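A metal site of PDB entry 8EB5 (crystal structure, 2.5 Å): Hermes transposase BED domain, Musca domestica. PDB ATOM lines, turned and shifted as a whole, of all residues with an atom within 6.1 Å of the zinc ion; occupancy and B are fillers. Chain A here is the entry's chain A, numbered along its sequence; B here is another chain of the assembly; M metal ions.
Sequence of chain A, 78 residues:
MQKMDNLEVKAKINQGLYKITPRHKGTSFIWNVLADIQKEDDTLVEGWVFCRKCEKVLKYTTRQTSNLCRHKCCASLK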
ATOM      1  N   VAL A  33      20.491 -22.426 -24.763  1.00  0.00           N
ATOM      2  CA  VAL A  33      19.396 -23.349 -24.492  1.00  0.00           C
ATOM      3  C   VAL A  33      18.096 -22.601 -24.117  1.00  0.00           C
ATOM      4  O   VAL A  33      17.015 -22.961 -24.573  1.00  0.00           O
ATOM      5  CB  VAL A  33      19.845 -24.318 -23.360  1.00  0.00           C
ATOM      6  CG1 VAL A  33      18.677 -25.044 -22.716  1.00  0.00           C
ATOM      7  CG2 VAL A  33      20.884 -25.306 -23.881  1.00  0.00           C
ATOM      8  N   LEU A  34      18.219 -21.577 -23.259  1.00  0.00           N
ATOM      9  CA  LEU A  34      17.090 -20.785 -22.761  1.00  0.00           C
ATOM     10  C   LEU A  34      16.749 -19.599 -23.682  1.00  0.00           C
ATOM     11  O   LEU A  34      17.652 -18.930 -24.189  1.00  0.00           O
ATOM     12  CB  LEU A  34      17.440 -20.246 -21.358  1.00  0.00           C
ATOM     13  CG  LEU A  34      17.090 -21.050 -20.080  1.00  0.00           C
ATOM     14  CD1 LEU A  34      16.892 -22.526 -20.314  1.00  0.00           C
ATOM     15  CD2 LEU A  34      18.153 -20.865 -19.075  1.00  0.00           C
ATOM     16  N   CYS A  51      12.916 -23.106 -21.754  1.00  0.00           N
ATOM     17  CA  CYS A  51      13.957 -24.033 -22.112  1.00  0.00           C
ATOM     18  C   CYS A  51      13.614 -24.722 -23.411  1.00  0.00           C
ATOM     19  O   CYS A  51      12.592 -25.381 -23.491  1.00  0.00           O
ATOM     20  CB  CYS A  51      14.238 -25.045 -21.016  1.00  0.00           C
ATOM     21  SG  CYS A  51      15.632 -26.117 -21.395  1.00  0.00           S
ATOM     22  N   ARG A  52      14.485 -24.617 -24.422  1.00  0.00           N
ATOM     23  CA  ARG A  52      14.234 -25.289 -25.702  1.00  0.00           C
ATOM     24  C   ARG A  52      14.302 -26.813 -25.599  1.00  0.00           C
ATOM     25  O   ARG A  52      13.594 -27.511 -26.320  1.00  0.00           O
ATOM     26  CB  ARG A  52      15.205 -24.789 -26.755  1.00  0.00           C
ATOM     27  CG  ARG A  52      14.896 -23.359 -27.154  1.00  0.00           C
ATOM     28  CD  ARG A  52      16.163 -22.633 -27.485  1.00  0.00           C
ATOM     29  NE  ARG A  52      15.896 -21.540 -28.401  1.00  0.00           N
ATOM     30  CZ  ARG A  52      16.682 -20.483 -28.559  1.00  0.00           C
ATOM     31  NH1 ARG A  52      17.804 -20.362 -27.852  1.00  0.00           N
ATOM     32  NH2 ARG A  52      16.353 -19.537 -29.432  1.00  0.00           N
ATOM     33  N   LYS A  53      15.110 -27.338 -24.667  1.00  0.00           N
ATOM     34  CA  LYS A  53      15.282 -28.774 -24.515  1.00  0.00           C
ATOM     35  C   LYS A  53      14.108 -29.470 -23.815  1.00  0.00           C
ATOM     36  O   LYS A  53      13.570 -30.414 -24.381  1.00  0.00           O
ATOM     37  CB  LYS A  53      16.618 -29.083 -23.828  1.00  0.00           C
ATOM     38  CG  LYS A  53      17.150 -30.479 -24.099  1.00  0.00           C
ATOM     39  CD  LYS A  53      18.584 -30.624 -23.608  1.00  0.00           C
ATOM     40  CE  LYS A  53      19.134 -32.019 -23.805  1.00  0.00           C
ATOM     41  NZ  LYS A  53      20.437 -32.207 -23.103  1.00  0.00           N
ATOM     42  N   CYS A  54      13.724 -29.063 -22.610  1.00  0.00           N
ATOM     43  CA  CYS A  54      12.633 -29.711 -21.871  1.00  0.00           C
ATOM     44  C   CYS A  54      11.253 -29.046 -22.091  1.00  0.00           C
ATOM     45  O   CYS A  54      10.223 -29.620 -21.723  1.00  0.00           O
ATOM     46  CB  CYS A  54      12.967 -29.821 -20.382  1.00  0.00           C
ATOM     47  SG  CYS A  54      13.082 -28.226 -19.506  1.00  0.00           S
ATOM     48  N   GLU A  55      11.257 -27.810 -22.644  1.00  0.00           N
ATOM     49  CA  GLU A  55      10.083 -26.983 -22.902  1.00  0.00           C
ATOM     50  C   GLU A  55       9.392 -26.502 -21.626  1.00  0.00           C
ATOM     51  O   GLU A  55       8.198 -26.213 -21.644  1.00  0.00           O
ATOM     52  CB  GLU A  55       9.119 -27.643 -23.880  1.00  0.00           C
ATOM     53  CG  GLU A  55       9.787 -27.844 -25.221  1.00  0.00           C
ATOM     54  CD  GLU A  55       8.885 -28.457 -26.270  1.00  0.00           C
ATOM     55  OE1 GLU A  55       8.021 -29.278 -25.883  1.00  0.00           O
ATOM     56  OE2 GLU A  55       9.034 -28.124 -27.468  1.00  0.00           O
ATOM     57  N   LYS A  56      10.149 -26.343 -20.541  1.00  0.00           N
ATOM     58  CA  LYS A  56       9.600 -25.809 -19.296  1.00  0.00           C
ATOM     59  C   LYS A  56       9.787 -24.285 -19.279  1.00  0.00           C
ATOM     60  O   LYS A  56      10.709 -23.748 -19.904  1.00  0.00           O
ATOM     61  CB  LYS A  56      10.307 -26.407 -18.063  1.00  0.00           C
ATOM     62  CG  LYS A  56       9.905 -27.808 -17.675  1.00  0.00           C
ATOM     63  CD  LYS A  56      10.585 -28.204 -16.342  1.00  0.00           C
ATOM     64  CE  LYS A  56      10.273 -29.618 -15.885  1.00  0.00           C
ATOM     65  NZ  LYS A  56      10.727 -29.883 -14.477  1.00  0.00           N
ATOM     66  N   LEU A  58      10.802 -21.322 -16.908  1.00  0.00           N
ATOM     67  CA  LEU A  58      11.545 -21.150 -15.661  1.00  0.00           C
ATOM     68  C   LEU A  58      11.578 -19.686 -15.214  1.00  0.00           C
ATOM     69  O   LEU A  58      11.620 -18.795 -16.043  1.00  0.00           O
ATOM     70  CB  LEU A  58      12.973 -21.691 -15.814  1.00  0.00           C
ATOM     71  CG  LEU A  58      13.126 -23.025 -16.537  1.00  0.00           C
ATOM     72  CD1 LEU A  58      14.417 -23.066 -17.317  1.00  0.00           C
ATOM     73  CD2 LEU A  58      12.988 -24.222 -15.567  1.00  0.00           C
ATOM     74  N   HIS A  71      19.917 -25.813 -13.892  1.00  0.00           N
ATOM     75  CA  HIS A  71      18.819 -26.495 -14.581  1.00  0.00           C
ATOM     76  C   HIS A  71      19.496 -27.522 -15.494  1.00  0.00           C
ATOM     77  O   HIS A  71      20.454 -27.168 -16.175  1.00  0.00           O
ATOM     78  CB  HIS A  71      18.054 -25.470 -15.422  1.00  0.00           C
ATOM     79  CG  HIS A  71      17.046 -26.088 -16.328  1.00  0.00           C
ATOM     80  ND1 HIS A  71      15.926 -26.728 -15.843  1.00  0.00           N
ATOM     81  CD2 HIS A  71      17.029 -26.160 -17.685  1.00  0.00           C
ATOM     82  CE1 HIS A  71      15.254 -27.140 -16.899  1.00  0.00           C
ATOM     83  NE2 HIS A  71      15.892 -26.857 -18.030  1.00  0.00           N
ATOM     84  N   LYS A  72      19.060 -28.795 -15.441  1.00  0.00           N
ATOM     85  CA  LYS A  72      19.776 -29.881 -16.084  1.00  0.00           C
ATOM     86  C   LYS A  72      20.153 -29.650 -17.521  1.00  0.00           C
ATOM     87  O   LYS A  72      21.282 -29.991 -17.883  1.00  0.00           O
ATOM     88  CB  LYS A  72      19.091 -31.253 -15.921  1.00  0.00           C
ATOM     89  CG  LYS A  72      17.593 -31.303 -16.153  1.00  0.00           C
ATOM     90  CD  LYS A  72      17.131 -32.764 -15.973  1.00  0.00           C
ATOM     91  CE  LYS A  72      15.653 -32.985 -16.200  1.00  0.00           C
ATOM     92  NZ  LYS A  72      15.315 -34.443 -16.238  1.00  0.00           N
ATOM     93  N   CYS A  73      19.307 -29.002 -18.295  1.00  0.00           N
ATOM     94  CA  CYS A  73      19.594 -28.777 -19.701  1.00  0.00           C
ATOM     95  C   CYS A  73      20.791 -27.818 -19.924  1.00  0.00           C
ATOM     96  O   CYS A  73      21.548 -28.018 -20.866  1.00  0.00           O
ATOM     97  CB  CYS A  73      18.334 -28.342 -20.443  1.00  0.00           C
ATOM     98  SG  CYS A  73      16.906 -29.431 -20.137  1.00  0.00           S
ATOM     99  N   CYS A  74      20.993 -26.837 -19.026  1.00  0.00           N
ATOM    100  CA  CYS A  74      22.131 -25.924 -19.141  1.00  0.00           C
ATOM    101  C   CYS A  74      23.376 -26.590 -18.569  1.00  0.00           C
ATOM    102  O   CYS A  74      24.447 -26.470 -19.153  1.00  0.00           O
ATOM    103  CB  CYS A  74      21.855 -24.624 -18.413  1.00  0.00           C
ATOM    104  SG  CYS A  74      20.307 -23.834 -18.879  1.00  0.00           S
ATOM    105  P    DC B   8      14.656 -28.501 -13.035  1.00  0.00           P
ATOM    106  OP1  DC B   8      13.771 -28.925 -14.155  1.00  0.00           O
ATOM    107  OP2  DC B   8      16.126 -28.563 -13.197  1.00  0.00           O
ATOM    108  O5'  DC B   8      14.274 -26.999 -12.574  1.00  0.00           O
ATOM    109  C5'  DC B   8      12.928 -26.534 -12.672  1.00  0.00           C
ATOM    110  C4'  DC B   8      12.367 -26.008 -11.343  1.00  0.00           C
ATOM    111  O4'  DC B   8      12.723 -26.853 -10.225  1.00  0.00           O
ATOM    112  C3'  DC B   8      12.825 -24.631 -10.894  1.00  0.00           C
ATOM    113  O3'  DC B   8      12.162 -23.600 -11.650  1.00  0.00           O
ATOM    114  C2'  DC B   8      12.326 -24.647  -9.449  1.00  0.00           C
ATOM    115  C1'  DC B   8      12.510 -26.112  -9.031  1.00  0.00           C
ATOM    116  N1   DC B   8      13.661 -26.301  -8.100  1.00  0.00           N
ATOM    117  C2   DC B   8      13.484 -26.041  -6.729  1.00  0.00           C
ATOM    118  O2   DC B   8      12.360 -25.730  -6.309  1.00  0.00           O
ATOM    119  N3   DC B   8      14.550 -26.177  -5.897  1.00  0.00           N
ATOM    120  C4   DC B   8      15.732 -26.511  -6.387  1.00  0.00           C
ATOM    121  N4   DC B   8      16.753 -26.625  -5.532  1.00  0.00           N
ATOM    122  C5   DC B   8      15.934 -26.762  -7.776  1.00  0.00           C
ATOM    123  C6   DC B   8      14.894 -26.617  -8.591  1.00  0.00           C
HETATM  124 ZN    ZN M   1      15.301 -27.771 -19.874  1.00  0.00          ZN
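OP2 of DC 8 of chain B lies within hydrogen-bond range of a ring nitrogen (ND1) of His 71.
The side-chain sulfur (SG) of Cys 51 lies close to the backbone NH (N) of Lys 53 (3.5 Å).
The backbone NH (N) of Cys 51 lies within hydrogen-bond range of the backbone carbonyl oxygen (O) of Lys 56, at 3.0 Å.
The backbone NH of Lys 56 lies close to the side-chain sulfur of Cys 54, 3.6 Å away.
The zinc ion is bound by a ring nitrogen (NE2) of His 71.
SG of Cys 51 is bound to the zinc ion, 2.3 Å away.
The side-chain sulfur (SG) of Cys 54 is bound to the zinc ion (2.3 Å).
The side-chain sulfur (SG) of Cys 73 is bound to the zinc ion, 2.3 Å away.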
